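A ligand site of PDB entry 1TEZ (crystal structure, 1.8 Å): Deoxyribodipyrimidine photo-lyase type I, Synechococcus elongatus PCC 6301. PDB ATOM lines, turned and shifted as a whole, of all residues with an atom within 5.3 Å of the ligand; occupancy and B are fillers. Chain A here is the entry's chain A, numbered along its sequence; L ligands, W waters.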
ATOM      1  N   TRP A   7      -8.269   4.411  14.160  1.00  0.00           N
ATOM      2  CA  TRP A   7      -7.830   5.729  13.754  1.00  0.00           C
ATOM      3  C   TRP A   7      -8.951   6.531  13.108  1.00  0.00           C
ATOM      4  O   TRP A   7      -9.402   6.224  12.012  1.00  0.00           O
ATOM      5  CB  TRP A   7      -6.629   5.564  12.817  1.00  0.00           C
ATOM      6  CG  TRP A   7      -6.065   6.840  12.226  1.00  0.00           C
ATOM      7  CD1 TRP A   7      -6.172   8.103  12.735  1.00  0.00           C
ATOM      8  CD2 TRP A   7      -5.309   6.947  11.024  1.00  0.00           C
ATOM      9  NE1 TRP A   7      -5.517   8.996  11.909  1.00  0.00           N
ATOM     10  CE2 TRP A   7      -4.980   8.314  10.850  1.00  0.00           C
ATOM     11  CE3 TRP A   7      -4.866   6.021  10.059  1.00  0.00           C
ATOM     12  CZ2 TRP A   7      -4.239   8.777   9.751  1.00  0.00           C
ATOM     13  CZ3 TRP A   7      -4.123   6.480   8.969  1.00  0.00           C
ATOM     14  CH2 TRP A   7      -3.823   7.850   8.825  1.00  0.00           C
ATOM     15  N   HIS A   8      -9.407   7.549  13.838  1.00  0.00           N
ATOM     16  CA  HIS A   8     -10.461   8.446  13.357  1.00  0.00           C
ATOM     17  C   HIS A   8      -9.848   9.577  12.541  1.00  0.00           C
ATOM     18  O   HIS A   8      -8.768  10.070  12.871  1.00  0.00           O
ATOM     19  CB  HIS A   8     -11.195   9.109  14.523  1.00  0.00           C
ATOM     20  CG  HIS A   8     -12.058   8.182  15.324  1.00  0.00           C
ATOM     21  ND1 HIS A   8     -13.362   7.908  14.982  1.00  0.00           N
ATOM     22  CD2 HIS A   8     -11.806   7.496  16.461  1.00  0.00           C
ATOM     23  CE1 HIS A   8     -13.879   7.084  15.878  1.00  0.00           C
ATOM     24  NE2 HIS A   8     -12.957   6.814  16.780  1.00  0.00           N
ATOM     25  N   ARG A   9     -10.550   9.980  11.485  1.00  0.00           N
ATOM     26  CA  ARG A   9     -10.091  11.101  10.657  1.00  0.00           C
ATOM     27  C   ARG A   9     -11.307  11.952  10.298  1.00  0.00           C
ATOM     28  O   ARG A   9     -11.383  13.128  10.661  1.00  0.00           O
ATOM     29  CB  ARG A   9      -9.386  10.613   9.385  1.00  0.00           C
ATOM     30  CG  ARG A   9      -8.161   9.742   9.662  1.00  0.00           C
ATOM     31  CD  ARG A   9      -8.549   8.261   9.705  1.00  0.00           C
ATOM     32  NE  ARG A   9      -8.994   7.827   8.377  1.00  0.00           N
ATOM     33  CZ  ARG A   9      -8.168   7.520   7.376  1.00  0.00           C
ATOM     34  NH1 ARG A   9      -6.851   7.580   7.542  1.00  0.00           N
ATOM     35  NH2 ARG A   9      -8.664   7.187   6.194  1.00  0.00           N
ATOM     36  N   ARG A  10     -12.290  11.358   9.619  1.00  0.00           N
ATOM     37  CA  ARG A  10     -13.495  12.107   9.259  1.00  0.00           C
ATOM     38  C   ARG A  10     -14.743  11.289   9.569  1.00  0.00           C
ATOM     39  O   ARG A  10     -15.717  11.310   8.829  1.00  0.00           O
ATOM     40  CB  ARG A  10     -13.455  12.505   7.773  1.00  0.00           C
ATOM     41  CG  ARG A  10     -13.246  11.361   6.791  1.00  0.00           C
ATOM     42  CD  ARG A  10     -13.107  11.898   5.373  1.00  0.00           C
ATOM     43  NE  ARG A  10     -14.268  12.699   4.976  1.00  0.00           N
ATOM     44  CZ  ARG A  10     -14.318  13.466   3.891  1.00  0.00           C
ATOM     45  NH1 ARG A  10     -13.272  13.551   3.083  1.00  0.00           N
ATOM     46  NH2 ARG A  10     -15.410  14.160   3.619  1.00  0.00           N
ATOM     47  N   PHE A  34      -6.684  10.011  17.173  1.00  0.00           N
ATOM     48  CA  PHE A  34      -6.853  11.090  16.199  1.00  0.00           C
ATOM     49  C   PHE A  34      -5.508  11.791  16.119  1.00  0.00           C
ATOM     50  O   PHE A  34      -4.888  12.079  17.138  1.00  0.00           O
ATOM     51  CB  PHE A  34      -7.911  12.100  16.611  1.00  0.00           C
ATOM     52  CG  PHE A  34      -8.199  13.122  15.547  1.00  0.00           C
ATOM     53  CD1 PHE A  34      -7.439  14.295  15.464  1.00  0.00           C
ATOM     54  CD2 PHE A  34      -9.164  12.889  14.564  1.00  0.00           C
ATOM     55  CE1 PHE A  34      -7.639  15.216  14.432  1.00  0.00           C
ATOM     56  CE2 PHE A  34      -9.368  13.797  13.527  1.00  0.00           C
ATOM     57  CZ  PHE A  34      -8.607  14.966  13.453  1.00  0.00           C
ATOM     58  N   CYS A  35      -5.059  12.081  14.900  1.00  0.00           N
ATOM     59  CA  CYS A  35      -3.769  12.736  14.714  1.00  0.00           C
ATOM     60  C   CYS A  35      -3.925  14.105  14.032  1.00  0.00           C
ATOM     61  O   CYS A  35      -4.269  14.181  12.847  1.00  0.00           O
ATOM     62  CB  CYS A  35      -2.858  11.831  13.879  1.00  0.00           C
ATOM     63  SG  CYS A  35      -1.151  12.439  13.692  1.00  0.00           S
ATOM     64  N   LEU A  36      -3.681  15.161  14.800  1.00  0.00           N
ATOM     65  CA  LEU A  36      -3.754  16.530  14.300  1.00  0.00           C
ATOM     66  C   LEU A  36      -2.618  16.620  13.282  1.00  0.00           C
ATOM     67  O   LEU A  36      -1.456  16.546  13.646  1.00  0.00           O
ATOM     68  CB  LEU A  36      -3.592  17.508  15.456  1.00  0.00           C
ATOM     69  CG  LEU A  36      -4.826  17.492  16.371  1.00  0.00           C
ATOM     70  CD1 LEU A  36      -4.510  18.136  17.709  1.00  0.00           C
ATOM     71  CD2 LEU A  36      -5.969  18.217  15.676  1.00  0.00           C
ATOM     72  N   ASP A  37      -3.008  16.773  12.020  1.00  0.00           N
ATOM     73  CA  ASP A  37      -2.105  16.770  10.881  1.00  0.00           C
ATOM     74  C   ASP A  37      -1.747  18.144  10.313  1.00  0.00           C
ATOM     75  O   ASP A  37      -2.589  18.807   9.712  1.00  0.00           O
ATOM     76  CB  ASP A  37      -2.771  15.920   9.784  1.00  0.00           C
ATOM     77  CG  ASP A  37      -1.849  15.594   8.639  1.00  0.00           C
ATOM     78  OD1 ASP A  37      -0.862  16.327   8.413  1.00  0.00           O
ATOM     79  OD2 ASP A  37      -2.132  14.592   7.954  1.00  0.00           O
ATOM     80  N   ILE A  40      -2.699  19.202   6.835  1.00  0.00           N
ATOM     81  CA  ILE A  40      -4.090  19.556   6.607  1.00  0.00           C
ATOM     82  C   ILE A  40      -4.417  20.865   7.309  1.00  0.00           C
ATOM     83  O   ILE A  40      -4.915  21.821   6.698  1.00  0.00           O
ATOM     84  CB  ILE A  40      -5.052  18.472   7.122  1.00  0.00           C
ATOM     85  CG1 ILE A  40      -4.779  17.138   6.406  1.00  0.00           C
ATOM     86  CG2 ILE A  40      -6.487  18.903   6.900  1.00  0.00           C
ATOM     87  CD1 ILE A  40      -5.585  15.954   6.954  1.00  0.00           C
ATOM     88  N   LEU A  41      -4.122  20.919   8.597  1.00  0.00           N
ATOM     89  CA  LEU A  41      -4.404  22.103   9.407  1.00  0.00           C
ATOM     90  C   LEU A  41      -3.725  23.396   8.942  1.00  0.00           C
ATOM     91  O   LEU A  41      -4.277  24.473   9.122  1.00  0.00           O
ATOM     92  CB  LEU A  41      -4.051  21.811  10.865  1.00  0.00           C
ATOM     93  CG  LEU A  41      -4.982  20.806  11.533  1.00  0.00           C
ATOM     94  CD1 LEU A  41      -4.411  20.370  12.884  1.00  0.00           C
ATOM     95  CD2 LEU A  41      -6.363  21.432  11.705  1.00  0.00           C
ATOM     96  N   MET A  46      -7.815  26.218   4.484  1.00  0.00           N
ATOM     97  CA  MET A  46      -8.434  25.830   5.751  1.00  0.00           C
ATOM     98  C   MET A  46      -9.325  26.977   6.239  1.00  0.00           C
ATOM     99  O   MET A  46      -8.990  28.147   6.061  1.00  0.00           O
ATOM    100  CB  MET A  46      -7.362  25.509   6.793  1.00  0.00           C
ATOM    101  CG  MET A  46      -7.893  24.937   8.093  1.00  0.00           C
ATOM    102  SD  MET A  46      -9.022  23.557   7.788  1.00  0.00           S
ATOM    103  CE  MET A  46      -7.988  22.475   6.846  1.00  0.00           C
ATOM    104  N   ARG A  50     -14.337  25.651  10.151  1.00  0.00           N
ATOM    105  CA  ARG A  50     -14.204  24.209   9.979  1.00  0.00           C
ATOM    106  C   ARG A  50     -13.344  23.615  11.086  1.00  0.00           C
ATOM    107  O   ARG A  50     -13.649  22.566  11.624  1.00  0.00           O
ATOM    108  CB  ARG A  50     -13.624  23.882   8.609  1.00  0.00           C
ATOM    109  CG  ARG A  50     -13.829  22.437   8.199  1.00  0.00           C
ATOM    110  CD  ARG A  50     -13.941  22.267   6.687  1.00  0.00           C
ATOM    111  NE  ARG A  50     -12.641  22.302   6.012  1.00  0.00           N
ATOM    112  CZ  ARG A  50     -12.196  23.324   5.283  1.00  0.00           C
ATOM    113  NH1 ARG A  50     -12.947  24.415   5.128  1.00  0.00           N
ATOM    114  NH2 ARG A  50     -11.023  23.242   4.684  1.00  0.00           N
ATOM    115  N   VAL A  51     -12.248  24.281  11.437  1.00  0.00           N
ATOM    116  CA  VAL A  51     -11.400  23.759  12.505  1.00  0.00           C
ATOM    117  C   VAL A  51     -12.141  23.843  13.843  1.00  0.00           C
ATOM    118  O   VAL A  51     -11.978  22.983  14.706  1.00  0.00           O
ATOM    119  CB  VAL A  51     -10.069  24.551  12.604  1.00  0.00           C
ATOM    120  CG1 VAL A  51      -9.210  23.962  13.702  1.00  0.00           C
ATOM    121  CG2 VAL A  51      -9.340  24.506  11.278  1.00  0.00           C
ATOM    122  N   LEU A  54     -14.494  20.922  13.958  1.00  0.00           N
ATOM    123  CA  LEU A  54     -13.688  19.740  14.181  1.00  0.00           C
ATOM    124  C   LEU A  54     -13.305  19.617  15.656  1.00  0.00           C
ATOM    125  O   LEU A  54     -13.467  18.581  16.290  1.00  0.00           O
ATOM    126  CB  LEU A  54     -12.404  19.816  13.347  1.00  0.00           C
ATOM    127  CG  LEU A  54     -11.275  18.862  13.759  1.00  0.00           C
ATOM    128  CD1 LEU A  54     -11.725  17.402  13.548  1.00  0.00           C
ATOM    129  CD2 LEU A  54     -10.038  19.162  12.952  1.00  0.00           C
ATOM    130  N   ASP A 100     -10.992   6.846   2.653  1.00  0.00           N
ATOM    131  CA  ASP A 100     -11.457   8.147   2.189  1.00  0.00           C
ATOM    132  C   ASP A 100     -11.306   8.187   0.672  1.00  0.00           C
ATOM    133  O   ASP A 100     -10.799   7.236   0.073  1.00  0.00           O
ATOM    134  CB  ASP A 100     -10.646   9.282   2.848  1.00  0.00           C
ATOM    135  CG  ASP A 100     -11.174  10.655   2.480  1.00  0.00           C
ATOM    136  OD1 ASP A 100     -12.415  10.786   2.323  1.00  0.00           O
ATOM    137  OD2 ASP A 100     -10.355  11.586   2.347  1.00  0.00           O
ATOM    138  N   GLU A 102     -10.204  11.287  -0.933  1.00  0.00           N
ATOM    139  CA  GLU A 102      -9.308  12.379  -1.316  1.00  0.00           C
ATOM    140  C   GLU A 102      -7.886  11.933  -1.618  1.00  0.00           C
ATOM    141  O   GLU A 102      -7.369  11.017  -0.966  1.00  0.00           O
ATOM    142  CB  GLU A 102      -9.278  13.440  -0.205  1.00  0.00           C
ATOM    143  CG  GLU A 102     -10.656  14.007   0.119  1.00  0.00           C
ATOM    144  CD  GLU A 102     -10.609  15.167   1.096  1.00  0.00           C
ATOM    145  OE1 GLU A 102      -9.499  15.488   1.591  1.00  0.00           O
ATOM    146  OE2 GLU A 102     -11.668  15.752   1.370  1.00  0.00           O
ATOM    147  N   TYR A 104      -4.897  13.256  -1.001  1.00  0.00           N
ATOM    148  CA  TYR A 104      -3.990  13.313   0.151  1.00  0.00           C
ATOM    149  C   TYR A 104      -4.247  12.154   1.104  1.00  0.00           C
ATOM    150  O   TYR A 104      -3.336  11.420   1.446  1.00  0.00           O
ATOM    151  CB  TYR A 104      -4.144  14.627   0.927  1.00  0.00           C
ATOM    152  CG  TYR A 104      -3.338  14.631   2.207  1.00  0.00           C
ATOM    153  CD1 TYR A 104      -1.947  14.743   2.179  1.00  0.00           C
ATOM    154  CD2 TYR A 104      -3.956  14.456   3.438  1.00  0.00           C
ATOM    155  CE1 TYR A 104      -1.184  14.663   3.341  1.00  0.00           C
ATOM    156  CE2 TYR A 104      -3.204  14.373   4.612  1.00  0.00           C
ATOM    157  CZ  TYR A 104      -1.821  14.482   4.562  1.00  0.00           C
ATOM    158  OH  TYR A 104      -1.079  14.380   5.715  1.00  0.00           O
ATOM    159  N   GLY A 105      -5.507  12.017   1.520  1.00  0.00           N
ATOM    160  CA  GLY A 105      -5.870  10.955   2.431  1.00  0.00           C
ATOM    161  C   GLY A 105      -5.542   9.558   1.946  1.00  0.00           C
ATOM    162  O   GLY A 105      -5.074   8.726   2.710  1.00  0.00           O
ATOM    163  N   ARG A 106      -5.783   9.281   0.677  1.00  0.00           N
ATOM    164  CA  ARG A 106      -5.506   7.939   0.163  1.00  0.00           C
ATOM    165  C   ARG A 106      -4.000   7.687   0.101  1.00  0.00           C
ATOM    166  O   ARG A 106      -3.533   6.582   0.395  1.00  0.00           O
ATOM    167  CB  ARG A 106      -6.161   7.742  -1.192  1.00  0.00           C
ATOM    168  CG  ARG A 106      -7.702   7.769  -1.130  1.00  0.00           C
ATOM    169  CD  ARG A 106      -8.334   7.200  -2.392  1.00  0.00           C
ATOM    170  NE  ARG A 106      -7.997   5.786  -2.576  1.00  0.00           N
ATOM    171  CZ  ARG A 106      -8.496   4.782  -1.862  1.00  0.00           C
ATOM    172  NH1 ARG A 106      -9.384   4.998  -0.886  1.00  0.00           N
ATOM    173  NH2 ARG A 106      -8.108   3.539  -2.113  1.00  0.00           N
ATOM    174  N   ARG A 108      -1.712   9.134   2.012  1.00  0.00           N
ATOM    175  CA  ARG A 108      -1.336   8.995   3.422  1.00  0.00           C
ATOM    176  C   ARG A 108      -1.643   7.586   3.927  1.00  0.00           C
ATOM    177  O   ARG A 108      -0.803   6.940   4.561  1.00  0.00           O
ATOM    178  CB  ARG A 108      -2.106  10.021   4.250  1.00  0.00           C
ATOM    179  CG  ARG A 108      -2.068   9.811   5.754  1.00  0.00           C
ATOM    180  CD  ARG A 108      -3.235  10.551   6.409  1.00  0.00           C
ATOM    181  NE  ARG A 108      -4.503  10.023   5.888  1.00  0.00           N
ATOM    182  CZ  ARG A 108      -5.683  10.597   6.064  1.00  0.00           C
ATOM    183  NH1 ARG A 108      -5.793  11.726   6.753  1.00  0.00           N
ATOM    184  NH2 ARG A 108      -6.776  10.047   5.521  1.00  0.00           N
ATOM    185  N   LYS A 247     -19.655  15.844   6.666  1.00  0.00           N
ATOM    186  CA  LYS A 247     -18.277  15.983   6.217  1.00  0.00           C
ATOM    187  C   LYS A 247     -17.328  15.297   7.200  1.00  0.00           C
ATOM    188  O   LYS A 247     -16.438  14.526   6.800  1.00  0.00           O
ATOM    189  CB  LYS A 247     -17.898  17.459   6.070  1.00  0.00           C
ATOM    190  CG  LYS A 247     -16.534  17.703   5.427  1.00  0.00           C
ATOM    191  CD  LYS A 247     -15.400  17.568   6.432  1.00  0.00           C
ATOM    192  CE  LYS A 247     -14.058  17.283   5.749  1.00  0.00           C
ATOM    193  NZ  LYS A 247     -13.672  18.321   4.752  1.00  0.00           N
ATOM    194  N   PHE A 248     -17.512  15.570   8.478  1.00  0.00           N
ATOM    195  CA  PHE A 248     -16.666  15.012   9.538  1.00  0.00           C
ATOM    196  C   PHE A 248     -17.207  13.712  10.146  1.00  0.00           C
ATOM    197  O   PHE A 248     -16.628  13.179  11.097  1.00  0.00           O
ATOM    198  CB  PHE A 248     -16.493  16.019  10.662  1.00  0.00           C
ATOM    199  CG  PHE A 248     -15.547  17.136  10.329  1.00  0.00           C
ATOM    200  CD1 PHE A 248     -14.177  16.926  10.339  1.00  0.00           C
ATOM    201  CD2 PHE A 248     -16.036  18.390   9.994  1.00  0.00           C
ATOM    202  CE1 PHE A 248     -13.291  17.957  10.039  1.00  0.00           C
ATOM    203  CE2 PHE A 248     -15.160  19.440   9.695  1.00  0.00           C
ATOM    204  CZ  PHE A 248     -13.782  19.214   9.717  1.00  0.00           C
ATOM    205  N   GLY A 380     -16.613  22.759   4.204  1.00  0.00           N
ATOM    206  CA  GLY A 380     -15.716  22.685   3.062  1.00  0.00           C
ATOM    207  C   GLY A 380     -15.229  21.260   2.833  1.00  0.00           C
ATOM    208  O   GLY A 380     -14.567  20.682   3.686  1.00  0.00           O
HETATM  209  N1  LIG L   1      -7.887  14.622   9.534  1.00  0.00           N
HETATM  210  C1  LIG L   1      -6.845  14.165  10.301  1.00  0.00           C
HETATM  211  O1  LIG L   1      -6.497  12.997  10.330  1.00  0.00           O
HETATM  212  N2  LIG L   1      -6.199  15.146  11.035  1.00  0.00           N
HETATM  213  C2  LIG L   1      -6.511  16.506  11.058  1.00  0.00           C
HETATM  214  O2  LIG L   1      -5.834  17.249  11.772  1.00  0.00           O
HETATM  215  C3  LIG L   1      -7.624  16.862  10.192  1.00  0.00           C
HETATM  216  C4  LIG L   1      -7.987  18.208  10.125  1.00  0.00           C
HETATM  217  C5  LIG L   1      -9.011  18.628   9.288  1.00  0.00           C
HETATM  218  C6  LIG L   1      -9.328  19.954   9.213  1.00  0.00           C
HETATM  219  C7  LIG L   1     -10.325  20.375   8.337  1.00  0.00           C
HETATM  220  C8  LIG L   1     -11.002  19.415   7.564  1.00  0.00           C
HETATM  221  O3  LIG L   1     -11.969  19.802   6.687  1.00  0.00           O
HETATM  222  C9  LIG L   1     -10.700  18.089   7.664  1.00  0.00           C
HETATM  223  C10 LIG L   1      -9.709  17.665   8.517  1.00  0.00           C
HETATM  224  N3  LIG L   1      -9.413  16.297   8.573  1.00  0.00           N
HETATM  225  C11 LIG L   1      -8.364  15.918   9.393  1.00  0.00           C
HETATM  226  C12 LIG L   1     -10.127  15.313   7.943  1.00  0.00           C
HETATM  227  C13 LIG L   1      -9.576  14.987   6.625  1.00  0.00           C
HETATM  228  O4  LIG L   1     -10.222  15.568   5.517  1.00  0.00           O
HETATM  229  C14 LIG L   1      -9.018  13.597   6.309  1.00  0.00           C
HETATM  230  O5  LIG L   1      -7.768  13.305   6.862  1.00  0.00           O
HETATM  231  C15 LIG L   1      -8.974  13.158   4.841  1.00  0.00           C
HETATM  232  O6  LIG L   1      -8.853  11.753   4.703  1.00  0.00           O
HETATM  233  C16 LIG L   1      -7.868  13.856   4.044  1.00  0.00           C
HETATM  234  O7  LIG L   1      -7.814  13.485   2.668  1.00  0.00           O
HETATM  235  O   HOH W   1      -6.538  11.541  12.557  1.00  0.00           O
HETATM  236  O   HOH W   2      -4.151  12.521   8.744  1.00  0.00           O
HETATM  237  O   HOH W   3      -9.690  17.156   3.684  1.00  0.00           O
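O5 of the ligand sits at hydrogen-bond distance from NH1 of Arg 108 (2.5 Å).
The guanidinium group (NE) of Arg 50 lies within hydrogen-bond range of an oxygen (O3) of the ligand (2.7 Å).
O6 of the ligand sits at hydrogen-bond distance from OD2 of Asp 100.
The backbone carbonyl oxygen (O) of Cys 35 sits at hydrogen-bond distance from a nitrogen (N2) of the ligand (2.8 Å).
An oxygen (O7) of the ligand is in hydrogen-bond range of the side-chain carboxylate of Glu 102, 2.8 Å away.
An oxygen (O2) of the ligand sits at hydrogen-bond distance from the backbone NH of Asp 37 (2.9 Å).
The backbone NH (N) of Gly 105 lies within hydrogen-bond range of an oxygen (O7) of the ligand, at 3.0 Å.
NZ of Lys 247 lies within hydrogen-bond range of O3 of the ligand, at 3.0 Å.
NE of Arg 108 is in hydrogen-bond range of O of Gly 105 (3.5 Å).
O of Gly 380 sits at hydrogen-bond distance from NE of Arg 50 (3.4 Å).
N of Glu 102 lies within hydrogen-bond range of OD2 of Asp 100 (3.3 Å).
NH1 of Arg 10 is in salt-bridge range of OD1 of Asp 100 (3.0 Å).
O of Asp 100 sits at hydrogen-bond distance from NH1 of Arg 106 (2.8 Å).
The guanidinium group (NH1) of Arg 10 is in salt-bridge range of the side-chain carboxylate (OE2) of Glu 102.
OD2 of Asp 37 is in hydrogen-bond range of OH of Tyr 104 (2.5 Å).
The backbone carbonyl oxygen of Lys 247 lies within hydrogen-bond range of the guanidinium group of Arg 10, at 3.4 Å.
Arg 9 touches the ligand.
Phe 34 touches the ligand (CZ to N2, 3.4 Å).
Leu 36 touches the ligand (CA to O2, 3.4 Å).
Ile 40 touches the ligand.
Leu 41 touches the ligand (CD1 to O2, 3.6 Å).
Met 46 touches the ligand (CE to C7, 3.5 Å).
Leu 54 touches the ligand (CD2 to C4, 3.6 Å).
Phe 248 touches the ligand (CE1 to C9, 3.5 Å).
Hydrophobic or aromatic side chains that line the ligand: Phe 34, Ile 40, Leu 41, Met 46, Leu 54 and Phe 248.
16 residues have an atom within 4 Å of the ligand: Arg 9, Phe 34, Cys 35, Leu 36, Asp 37, Ile 40, Leu 41, Met 46, Arg 50, Leu 54, Asp 100, Glu 102, Gly 105, Arg 108, Lys 247 and Phe 248.
Water W3 lies within hydrogen-bond range of an oxygen (O4) of the ligand and the side-chain carboxylate of Glu 102.
Water W1 lies within hydrogen-bond range of O1 of the ligand (2.7 Å), O of His 8 (2.7 Å), NE1 of Trp 7 (2.8 Å) and N of Cys 35 (2.8 Å).
Water W2 lies within hydrogen-bond range of NH1 of Arg 108 (2.7 Å), O1 of the ligand (2.9 Å) and OD2 of Asp 37 (3.0 Å).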
